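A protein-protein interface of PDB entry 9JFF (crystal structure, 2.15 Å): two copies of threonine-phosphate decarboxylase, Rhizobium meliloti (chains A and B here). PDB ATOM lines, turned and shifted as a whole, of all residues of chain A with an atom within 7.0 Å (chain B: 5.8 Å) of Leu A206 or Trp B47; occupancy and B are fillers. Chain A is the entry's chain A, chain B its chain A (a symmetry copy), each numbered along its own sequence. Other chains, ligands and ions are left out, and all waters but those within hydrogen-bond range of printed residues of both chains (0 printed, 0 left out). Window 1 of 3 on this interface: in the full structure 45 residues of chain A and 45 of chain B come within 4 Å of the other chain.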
ATOM      1  N   PRO A  36      -1.136   6.570 -27.940  1.00  0.00           N
ATOM      2  CA  PRO A  36      -0.696   5.175 -28.058  1.00  0.00           C
ATOM      3  C   PRO A  36      -1.512   4.409 -29.088  1.00  0.00           C
ATOM      4  O   PRO A  36      -2.726   4.589 -29.217  1.00  0.00           O
ATOM      5  CB  PRO A  36      -0.897   4.615 -26.645  1.00  0.00           C
ATOM      6  CG  PRO A  36      -1.881   5.547 -25.989  1.00  0.00           C
ATOM      7  CD  PRO A  36      -1.602   6.897 -26.581  1.00  0.00           C
ATOM      8  N   LEU A  39      -3.858  -1.671 -28.791  1.00  0.00           N
ATOM      9  CA  LEU A  39      -3.150  -2.894 -28.414  1.00  0.00           C
ATOM     10  C   LEU A  39      -3.528  -4.050 -29.333  1.00  0.00           C
ATOM     11  O   LEU A  39      -4.717  -4.315 -29.529  1.00  0.00           O
ATOM     12  CB  LEU A  39      -3.473  -3.278 -26.976  1.00  0.00           C
ATOM     13  CG  LEU A  39      -2.743  -2.559 -25.852  1.00  0.00           C
ATOM     14  CD1 LEU A  39      -3.111  -3.215 -24.540  1.00  0.00           C
ATOM     15  CD2 LEU A  39      -1.238  -2.600 -26.086  1.00  0.00           C
ATOM     16  N   VAL A  42      -3.068 -10.305 -27.412  1.00  0.00           N
ATOM     17  CA  VAL A  42      -2.025 -11.050 -26.724  1.00  0.00           C
ATOM     18  C   VAL A  42      -2.639 -12.336 -26.184  1.00  0.00           C
ATOM     19  O   VAL A  42      -3.349 -12.322 -25.178  1.00  0.00           O
ATOM     20  CB  VAL A  42      -1.383 -10.227 -25.592  1.00  0.00           C
ATOM     21  CG1 VAL A  42      -0.366 -11.073 -24.849  1.00  0.00           C
ATOM     22  CG2 VAL A  42      -0.713  -8.992 -26.155  1.00  0.00           C
ATOM     23  N   TRP A  47       0.942 -14.758 -22.031  1.00  0.00           N
ATOM     24  CA  TRP A  47       0.945 -14.313 -20.639  1.00  0.00           C
ATOM     25  C   TRP A  47       1.449 -15.399 -19.695  1.00  0.00           C
ATOM     26  O   TRP A  47       2.135 -15.101 -18.708  1.00  0.00           O
ATOM     27  CB  TRP A  47      -0.464 -13.904 -20.211  1.00  0.00           C
ATOM     28  CG  TRP A  47      -0.972 -12.639 -20.818  1.00  0.00           C
ATOM     29  CD1 TRP A  47      -1.837 -12.521 -21.868  1.00  0.00           C
ATOM     30  CD2 TRP A  47      -0.667 -11.308 -20.396  1.00  0.00           C
ATOM     31  NE1 TRP A  47      -2.078 -11.196 -22.134  1.00  0.00           N
ATOM     32  CE2 TRP A  47      -1.369 -10.430 -21.246  1.00  0.00           C
ATOM     33  CE3 TRP A  47       0.140 -10.772 -19.388  1.00  0.00           C
ATOM     34  CZ2 TRP A  47      -1.297  -9.046 -21.113  1.00  0.00           C
ATOM     35  CZ3 TRP A  47       0.214  -9.395 -19.262  1.00  0.00           C
ATOM     36  CH2 TRP A  47      -0.500  -8.549 -20.118  1.00  0.00           C
ATOM     37  N   PRO A  78      15.141  -5.739 -22.748  1.00  0.00           N
ATOM     38  CA  PRO A  78      14.029  -5.163 -21.956  1.00  0.00           C
ATOM     39  C   PRO A  78      14.209  -3.665 -21.722  1.00  0.00           C
ATOM     40  O   PRO A  78      14.433  -3.186 -20.609  1.00  0.00           O
ATOM     41  CB  PRO A  78      14.089  -5.986 -20.663  1.00  0.00           C
ATOM     42  CG  PRO A  78      15.563  -6.313 -20.503  1.00  0.00           C
ATOM     43  CD  PRO A  78      16.118  -6.463 -21.910  1.00  0.00           C
ATOM     44  N   GLY A  79      14.091  -2.890 -22.799  1.00  0.00           N
ATOM     45  CA  GLY A  79      14.381  -1.471 -22.746  1.00  0.00           C
ATOM     46  C   GLY A  79      15.843  -1.211 -23.046  1.00  0.00           C
ATOM     47  O   GLY A  79      16.710  -1.968 -22.586  1.00  0.00           O
ATOM     48  N   PHE A 197      11.475   0.884 -28.467  1.00  0.00           N
ATOM     49  CA  PHE A 197      10.122   0.629 -28.944  1.00  0.00           C
ATOM     50  C   PHE A 197       9.102   1.607 -28.379  1.00  0.00           C
ATOM     51  O   PHE A 197       8.114   1.917 -29.056  1.00  0.00           O
ATOM     52  CB  PHE A 197       9.708  -0.805 -28.596  1.00  0.00           C
ATOM     53  CG  PHE A 197       8.335  -1.193 -29.102  1.00  0.00           C
ATOM     54  CD1 PHE A 197       8.135  -1.522 -30.440  1.00  0.00           C
ATOM     55  CD2 PHE A 197       7.255  -1.258 -28.235  1.00  0.00           C
ATOM     56  CE1 PHE A 197       6.878  -1.895 -30.904  1.00  0.00           C
ATOM     57  CE2 PHE A 197       5.995  -1.630 -28.690  1.00  0.00           C
ATOM     58  CZ  PHE A 197       5.805  -1.945 -30.021  1.00  0.00           C
ATOM     59  N   GLY A 198       9.331   2.122 -27.170  1.00  0.00           N
ATOM     60  CA  GLY A 198       8.273   2.834 -26.467  1.00  0.00           C
ATOM     61  C   GLY A 198       7.913   4.181 -27.074  1.00  0.00           C
ATOM     62  O   GLY A 198       6.737   4.547 -27.127  1.00  0.00           O
ATOM     63  N   GLY A 202       4.298   4.687 -28.570  1.00  0.00           N
ATOM     64  CA  GLY A 202       3.515   5.190 -27.461  1.00  0.00           C
ATOM     65  C   GLY A 202       3.163   4.154 -26.424  1.00  0.00           C
ATOM     66  O   GLY A 202       2.171   4.312 -25.714  1.00  0.00           O
ATOM     67  N   LEU A 203       3.943   3.083 -26.323  1.00  0.00           N
ATOM     68  CA  LEU A 203       3.690   2.055 -25.324  1.00  0.00           C
ATOM     69  C   LEU A 203       4.894   1.926 -24.400  1.00  0.00           C
ATOM     70  O   LEU A 203       5.517   0.862 -24.318  1.00  0.00           O
ATOM     71  CB  LEU A 203       3.374   0.725 -26.008  1.00  0.00           C
ATOM     72  CG  LEU A 203       2.082   0.735 -26.818  1.00  0.00           C
ATOM     73  CD1 LEU A 203       1.936  -0.569 -27.570  1.00  0.00           C
ATOM     74  CD2 LEU A 203       0.880   0.978 -25.906  1.00  0.00           C
ATOM     75  N   ALA A 204       5.239   3.012 -23.714  1.00  0.00           N
ATOM     76  CA  ALA A 204       6.432   3.034 -22.879  1.00  0.00           C
ATOM     77  C   ALA A 204       6.237   2.304 -21.558  1.00  0.00           C
ATOM     78  O   ALA A 204       7.199   2.176 -20.792  1.00  0.00           O
ATOM     79  CB  ALA A 204       6.871   4.479 -22.619  1.00  0.00           C
ATOM     80  N   GLY A 205       5.019   1.844 -21.264  1.00  0.00           N
ATOM     81  CA  GLY A 205       4.830   0.947 -20.138  1.00  0.00           C
ATOM     82  C   GLY A 205       5.459  -0.405 -20.378  1.00  0.00           C
ATOM     83  O   GLY A 205       5.867  -1.078 -19.427  1.00  0.00           O
ATOM     84  N   LEU A 206       5.543  -0.819 -21.641  1.00  0.00           N
ATOM     85  CA  LEU A 206       6.344  -1.971 -22.032  1.00  0.00           C
ATOM     86  C   LEU A 206       7.816  -1.595 -22.018  1.00  0.00           C
ATOM     87  O   LEU A 206       8.193  -0.487 -22.408  1.00  0.00           O
ATOM     88  CB  LEU A 206       5.965  -2.454 -23.434  1.00  0.00           C
ATOM     89  CG  LEU A 206       4.594  -3.083 -23.652  1.00  0.00           C
ATOM     90  CD1 LEU A 206       4.416  -3.456 -25.115  1.00  0.00           C
ATOM     91  CD2 LEU A 206       4.454  -4.301 -22.766  1.00  0.00           C
ATOM     92  N   ARG A 207       8.653  -2.516 -21.585  1.00  0.00           N
ATOM     93  CA  ARG A 207      10.091  -2.276 -21.550  1.00  0.00           C
ATOM     94  C   ARG A 207      10.709  -3.104 -22.673  1.00  0.00           C
ATOM     95  O   ARG A 207      10.941  -4.307 -22.514  1.00  0.00           O
ATOM     96  CB  ARG A 207      10.648  -2.619 -20.172  1.00  0.00           C
ATOM     97  CG  ARG A 207       9.879  -1.929 -19.042  1.00  0.00           C
ATOM     98  CD  ARG A 207       9.875  -0.391 -19.187  1.00  0.00           C
ATOM     99  NE  ARG A 207      11.231   0.150 -19.216  1.00  0.00           N
ATOM    100  CZ  ARG A 207      11.733   0.897 -20.193  1.00  0.00           C
ATOM    101  NH1 ARG A 207      10.984   1.314 -21.205  1.00  0.00           N
ATOM    102  NH2 ARG A 207      13.017   1.236 -20.154  1.00  0.00           N
ATOM    103  N   LEU A 208      10.944  -2.464 -23.821  1.00  0.00           N
ATOM    104  CA  LEU A 208      11.429  -3.183 -24.995  1.00  0.00           C
ATOM    105  C   LEU A 208      12.284  -2.285 -25.879  1.00  0.00           C
ATOM    106  O   LEU A 208      11.884  -1.169 -26.226  1.00  0.00           O
ATOM    107  CB  LEU A 208      10.267  -3.747 -25.813  1.00  0.00           C
ATOM    108  CG  LEU A 208      10.663  -4.431 -27.124  1.00  0.00           C
ATOM    109  CD1 LEU A 208      11.503  -5.686 -26.873  1.00  0.00           C
ATOM    110  CD2 LEU A 208       9.427  -4.757 -27.935  1.00  0.00           C
ATOM    111  N   GLY A 209      13.460  -2.790 -26.243  1.00  0.00           N
ATOM    112  CA  GLY A 209      14.285  -2.190 -27.268  1.00  0.00           C
ATOM    113  C   GLY A 209      14.916  -3.287 -28.100  1.00  0.00           C
ATOM    114  O   GLY A 209      14.650  -4.471 -27.889  1.00  0.00           O
ATOM    115  N   SER A 231       9.655  -9.736 -21.848  1.00  0.00           N
ATOM    116  CA  SER A 231       8.385 -10.368 -21.527  1.00  0.00           C
ATOM    117  C   SER A 231       7.690 -10.905 -22.778  1.00  0.00           C
ATOM    118  O   SER A 231       7.899 -10.422 -23.894  1.00  0.00           O
ATOM    119  CB  SER A 231       7.465  -9.379 -20.809  1.00  0.00           C
ATOM    120  OG  SER A 231       6.786  -8.544 -21.735  1.00  0.00           O
ATOM    121  N   PRO A 233       4.359 -10.706 -23.459  1.00  0.00           N
ATOM    122  CA  PRO A 233       3.501  -9.659 -24.046  1.00  0.00           C
ATOM    123  C   PRO A 233       4.256  -8.644 -24.890  1.00  0.00           C
ATOM    124  O   PRO A 233       3.789  -8.304 -25.985  1.00  0.00           O
ATOM    125  CB  PRO A 233       2.853  -9.013 -22.811  1.00  0.00           C
ATOM    126  CG  PRO A 233       2.783 -10.112 -21.820  1.00  0.00           C
ATOM    127  CD  PRO A 233       4.062 -10.910 -22.026  1.00  0.00           C
ATOM    128  N   ALA A 234       5.414  -8.159 -24.422  1.00  0.00           N
ATOM    129  CA  ALA A 234       6.187  -7.187 -25.197  1.00  0.00           C
ATOM    130  C   ALA A 234       6.589  -7.749 -26.560  1.00  0.00           C
ATOM    131  O   ALA A 234       6.478  -7.064 -27.587  1.00  0.00           O
ATOM    132  CB  ALA A 234       7.429  -6.752 -24.410  1.00  0.00           C
ATOM    133  N   LEU A 235       7.062  -8.999 -26.592  1.00  0.00           N
ATOM    134  CA  LEU A 235       7.483  -9.598 -27.856  1.00  0.00           C
ATOM    135  C   LEU A 235       6.297  -9.864 -28.776  1.00  0.00           C
ATOM    136  O   LEU A 235       6.435  -9.802 -30.003  1.00  0.00           O
ATOM    137  CB  LEU A 235       8.234 -10.905 -27.594  1.00  0.00           C
ATOM    138  CG  LEU A 235       9.540 -10.848 -26.805  1.00  0.00           C
ATOM    139  CD1 LEU A 235       9.912 -12.234 -26.294  1.00  0.00           C
ATOM    140  CD2 LEU A 235      10.644 -10.291 -27.676  1.00  0.00           C
ATOM    141  N   ILE A 237       3.414  -8.050 -28.790  1.00  0.00           N
ATOM    142  CA  ILE A 237       2.879  -6.769 -29.221  1.00  0.00           C
ATOM    143  C   ILE A 237       3.767  -6.143 -30.291  1.00  0.00           C
ATOM    144  O   ILE A 237       3.269  -5.605 -31.288  1.00  0.00           O
ATOM    145  CB  ILE A 237       2.699  -5.855 -27.994  1.00  0.00           C
ATOM    146  CG1 ILE A 237       1.498  -6.333 -27.169  1.00  0.00           C
ATOM    147  CG2 ILE A 237       2.562  -4.387 -28.403  1.00  0.00           C
ATOM    148  CD1 ILE A 237       1.451  -5.777 -25.757  1.00  0.00           C
ATOM    149  N   SER A 238       5.091  -6.217 -30.122  1.00  0.00           N
ATOM    150  CA  SER A 238       5.963  -5.538 -31.077  1.00  0.00           C
ATOM    151  C   SER A 238       5.922  -6.209 -32.444  1.00  0.00           C
ATOM    152  O   SER A 238       5.998  -5.529 -33.472  1.00  0.00           O
ATOM    153  CB  SER A 238       7.396  -5.482 -30.560  1.00  0.00           C
ATOM    154  OG  SER A 238       8.035  -6.739 -30.661  1.00  0.00           O
ATOM    155  N   LEU A 241       2.604  -4.867 -34.086  1.00  0.00           N
ATOM    156  CA  LEU A 241       2.606  -3.447 -34.435  1.00  0.00           C
ATOM    157  C   LEU A 241       3.619  -3.134 -35.530  1.00  0.00           C
ATOM    158  O   LEU A 241       3.349  -2.308 -36.410  1.00  0.00           O
ATOM    159  CB  LEU A 241       2.884  -2.594 -33.196  1.00  0.00           C
ATOM    160  CG  LEU A 241       1.801  -2.594 -32.114  1.00  0.00           C
ATOM    161  CD1 LEU A 241       2.148  -1.607 -31.016  1.00  0.00           C
ATOM    162  CD2 LEU A 241       0.426  -2.283 -32.699  1.00  0.00           C
ATOM    163  N   VAL B  42      -5.824  -3.768 -16.806  1.00  0.00           N
ATOM    164  CA  VAL B  42      -4.633  -2.946 -16.962  1.00  0.00           C
ATOM    165  C   VAL B  42      -5.019  -1.695 -17.740  1.00  0.00           C
ATOM    166  O   VAL B  42      -5.197  -1.739 -18.958  1.00  0.00           O
ATOM    167  CB  VAL B  42      -3.498  -3.709 -17.670  1.00  0.00           C
ATOM    168  CG1 VAL B  42      -2.312  -2.787 -17.886  1.00  0.00           C
ATOM    169  CG2 VAL B  42      -3.075  -4.906 -16.845  1.00  0.00           C
ATOM    170  N   PRO B  43      -5.155  -0.553 -17.061  1.00  0.00           N
ATOM    171  CA  PRO B  43      -5.590   0.667 -17.749  1.00  0.00           C
ATOM    172  C   PRO B  43      -4.606   1.083 -18.827  1.00  0.00           C
ATOM    173  O   PRO B  43      -3.409   0.791 -18.758  1.00  0.00           O
ATOM    174  CB  PRO B  43      -5.653   1.704 -16.622  1.00  0.00           C
ATOM    175  CG  PRO B  43      -5.784   0.902 -15.379  1.00  0.00           C
ATOM    176  CD  PRO B  43      -4.985  -0.338 -15.618  1.00  0.00           C
ATOM    177  N   GLU B  44      -5.139   1.767 -19.841  1.00  0.00           N
ATOM    178  CA  GLU B  44      -4.309   2.223 -20.949  1.00  0.00           C
ATOM    179  C   GLU B  44      -3.130   3.055 -20.460  1.00  0.00           C
ATOM    180  O   GLU B  44      -2.036   2.981 -21.032  1.00  0.00           O
ATOM    181  CB  GLU B  44      -5.159   3.025 -21.931  1.00  0.00           C
ATOM    182  CG  GLU B  44      -4.381   3.643 -23.080  1.00  0.00           C
ATOM    183  CD  GLU B  44      -5.242   4.567 -23.917  1.00  0.00           C
ATOM    184  OE1 GLU B  44      -6.418   4.222 -24.156  1.00  0.00           O
ATOM    185  OE2 GLU B  44      -4.747   5.642 -24.318  1.00  0.00           O
ATOM    186  N   ARG B  45      -3.332   3.838 -19.399  1.00  0.00           N
ATOM    187  CA  ARG B  45      -2.248   4.633 -18.837  1.00  0.00           C
ATOM    188  C   ARG B  45      -1.042   3.760 -18.491  1.00  0.00           C
ATOM    189  O   ARG B  45       0.101   4.123 -18.791  1.00  0.00           O
ATOM    190  CB  ARG B  45      -2.758   5.384 -17.608  1.00  0.00           C
ATOM    191  CG  ARG B  45      -1.909   6.561 -17.188  1.00  0.00           C
ATOM    192  CD  ARG B  45      -2.537   7.312 -16.013  1.00  0.00           C
ATOM    193  NE  ARG B  45      -1.610   8.280 -15.436  1.00  0.00           N
ATOM    194  CZ  ARG B  45      -1.474   9.535 -15.849  1.00  0.00           C
ATOM    195  NH1 ARG B  45      -2.209  10.023 -16.837  1.00  0.00           N
ATOM    196  NH2 ARG B  45      -0.580  10.321 -15.251  1.00  0.00           N
ATOM    197  N   ALA B  46      -1.283   2.586 -17.893  1.00  0.00           N
ATOM    198  CA  ALA B  46      -0.185   1.698 -17.512  1.00  0.00           C
ATOM    199  C   ALA B  46       0.564   1.159 -18.726  1.00  0.00           C
ATOM    200  O   ALA B  46       1.762   0.870 -18.630  1.00  0.00           O
ATOM    201  CB  ALA B  46      -0.713   0.542 -16.661  1.00  0.00           C
ATOM    202  N   TRP B  47      -0.116   1.018 -19.869  1.00  0.00           N
ATOM    203  CA  TRP B  47       0.543   0.597 -21.103  1.00  0.00           C
ATOM    204  C   TRP B  47       1.348   1.727 -21.734  1.00  0.00           C
ATOM    205  O   TRP B  47       2.422   1.490 -22.301  1.00  0.00           O
ATOM    206  CB  TRP B  47      -0.491   0.104 -22.113  1.00  0.00           C
ATOM    207  CG  TRP B  47      -1.135  -1.201 -21.782  1.00  0.00           C
ATOM    208  CD1 TRP B  47      -2.371  -1.391 -21.233  1.00  0.00           C
ATOM    209  CD2 TRP B  47      -0.586  -2.502 -22.000  1.00  0.00           C
ATOM    210  NE1 TRP B  47      -2.620  -2.733 -21.084  1.00  0.00           N
ATOM    211  CE2 TRP B  47      -1.538  -3.438 -21.544  1.00  0.00           C
ATOM    212  CE3 TRP B  47       0.621  -2.969 -22.527  1.00  0.00           C
ATOM    213  CZ2 TRP B  47      -1.324  -4.812 -21.609  1.00  0.00           C
ATOM    214  CZ3 TRP B  47       0.833  -4.337 -22.585  1.00  0.00           C
ATOM    215  CH2 TRP B  47      -0.134  -5.240 -22.130  1.00  0.00           C
ATOM    216  N   HIS B  48       0.832   2.956 -21.644  1.00  0.00           N
ATOM    217  CA  HIS B  48       1.334   4.083 -22.426  1.00  0.00           C
ATOM    218  C   HIS B  48       2.552   4.738 -21.773  1.00  0.00           C
ATOM    219  O   HIS B  48       3.559   4.995 -22.440  1.00  0.00           O
ATOM    220  CB  HIS B  48       0.207   5.104 -22.614  1.00  0.00           C
ATOM    221  CG  HIS B  48       0.644   6.392 -23.245  1.00  0.00           C
ATOM    222  ND1 HIS B  48       0.428   7.620 -22.653  1.00  0.00           N
ATOM    223  CD2 HIS B  48       1.266   6.647 -24.422  1.00  0.00           C
ATOM    224  CE1 HIS B  48       0.908   8.572 -23.434  1.00  0.00           C
ATOM    225  NE2 HIS B  48       1.418   8.009 -24.515  1.00  0.00           N
ATOM    226  N   ARG B  49       2.476   5.007 -20.475  1.00  0.00           N
ATOM    227  CA  ARG B  49       3.484   5.796 -19.782  1.00  0.00           C
ATOM    228  C   ARG B  49       4.658   4.942 -19.312  1.00  0.00           C
ATOM    229  O   ARG B  49       4.502   3.766 -18.970  1.00  0.00           O
ATOM    230  CB  ARG B  49       2.868   6.498 -18.569  1.00  0.00           C
ATOM    231  CG  ARG B  49       1.703   7.418 -18.892  1.00  0.00           C
ATOM    232  CD  ARG B  49       1.216   8.110 -17.630  1.00  0.00           C
ATOM    233  NE  ARG B  49       2.318   8.672 -16.856  1.00  0.00           N
ATOM    234  CZ  ARG B  49       2.903   9.834 -17.123  1.00  0.00           C
ATOM    235  NH1 ARG B  49       2.513  10.588 -18.140  1.00  0.00           N
ATOM    236  NH2 ARG B  49       3.909  10.246 -16.356  1.00  0.00           N
ATOM    237  N   SER B 231       8.049  -3.423 -16.024  1.00  0.00           N
ATOM    238  CA  SER B 231       7.022  -2.870 -16.894  1.00  0.00           C
ATOM    239  C   SER B 231       5.804  -2.399 -16.099  1.00  0.00           C
ATOM    240  O   SER B 231       5.518  -2.885 -15.001  1.00  0.00           O
ATOM    241  CB  SER B 231       6.591  -3.906 -17.933  1.00  0.00           C
ATOM    242  OG  SER B 231       5.623  -4.797 -17.401  1.00  0.00           O
ATOM    243  N   GLY B 232       5.088  -1.430 -16.673  1.00  0.00           N
ATOM    244  CA  GLY B 232       3.844  -0.943 -16.119  1.00  0.00           C
ATOM    245  C   GLY B 232       2.804  -2.035 -15.938  1.00  0.00           C
ATOM    246  O   GLY B 232       2.216  -2.178 -14.861  1.00  0.00           O
ATOM    247  N   PRO B 233       2.544  -2.825 -16.990  1.00  0.00           N
ATOM    248  CA  PRO B 233       1.584  -3.934 -16.838  1.00  0.00           C
ATOM    249  C   PRO B 233       1.942  -4.910 -15.728  1.00  0.00           C
ATOM    250  O   PRO B 233       1.054  -5.297 -14.956  1.00  0.00           O
ATOM    251  CB  PRO B 233       1.606  -4.602 -18.221  1.00  0.00           C
ATOM    252  CG  PRO B 233       1.919  -3.494 -19.154  1.00  0.00           C
ATOM    253  CD  PRO B 233       2.913  -2.618 -18.406  1.00  0.00           C
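N of Ala A204 is in hydrogen-bond range of O of His B48, 2.9 Å away. The backbone carbonyl oxygen (O) of Trp B47 is in hydrogen-bond range of the backbone NH (N) of Gly A205, 2.8 Å away. The backbone NH (N) of Gly A205 is in hydrogen-bond range of the backbone carbonyl oxygen (O) of Arg B49, at 3.0 Å. O of Gly A205 lies within hydrogen-bond range of N of Gly B232 (2.9 Å). The backbone carbonyl oxygen (O) of Trp B47 lies close to the backbone NH (N) of Ala A204 (3.5 Å).
NE1 of Trp A47 lies close to O of Val A42, at 3.5 Å. N of Gly A79 sits close to O of Arg A207, at 3.5 Å. The backbone NH (N) of Leu A203 lies within hydrogen-bond range of the backbone carbonyl oxygen (O) of Gly A198. The indole nitrogen (NE1) of Trp B47 sits close to the backbone carbonyl oxygen (O) of Val B42.
Glu B44 touches Pro A36. Pro A36 touches His B48 (CD to CD2, 3.6 Å). Leu A39 touches Trp B47 (CD1 to CE2, 3.4 Å). Trp B47 touches Trp A47 (CH2 to CH2, 3.9 Å). Gly A202 touches His B48 (O to CD2, 2.8 Å). O of Trp B47 touches C of Leu A203, at 3.3 Å. Leu A203 touches His B48. Ala A204 touches Arg B49 (C to O, 3.4 Å). CA of Ser B231 touches CG of Arg A207 (3.7 Å). Trp B47 touches Ile A237 (CZ3 to CD1, 3.5 Å).
Printed residues of chain B within 4 Å of Leu A39: Trp B47 (3.4 Å). Leu A206 touches one residue of chain B. Leu A241 touches none of the printed residues of chain B. Pro B43 touches none of the printed residues of chain A. Printed residues of chain A within 4 Å of Trp B47: Leu A39, Trp A47, Leu A203, Ala A204, Gly A205, Leu A206 and Ile A237. Printed residues of chain A within 4 Å of Arg B49: Ala A204 and Gly A205. The nearest residue of chain B that does not touch Leu A206 is Pro B233 (4.5 Å). The nearest printed residue of chain B that does not touch Ala A204 is Ala B46 (5.5 Å).
Of the 23 printed residues of chain A, 10 touch a printed residue of chain B. Hydrophobic or aromatic side chains of chain A that line the printed part of chain B: Pro A36, Leu A39, Trp A47, Leu A203, Ala A204, Leu A206 and Ile A237. Printed residues of chain B that touch a printed residue of chain A: Glu B44, Ala B46, Trp B47, His B48, Arg B49, Ser B231, Gly B232 and Pro B233. Hydrophobic or aromatic side chains of chain B that line the printed part of chain A: Trp B47, His B48 and Pro B233. Among the printed residues, 20 pairs touch across the chains.
Trp A47 touches its own counterpart, Trp B47. Of the 20 pairs that touch across the chains among the printed residues, 1 has its exchanged pair printed and touching as well.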
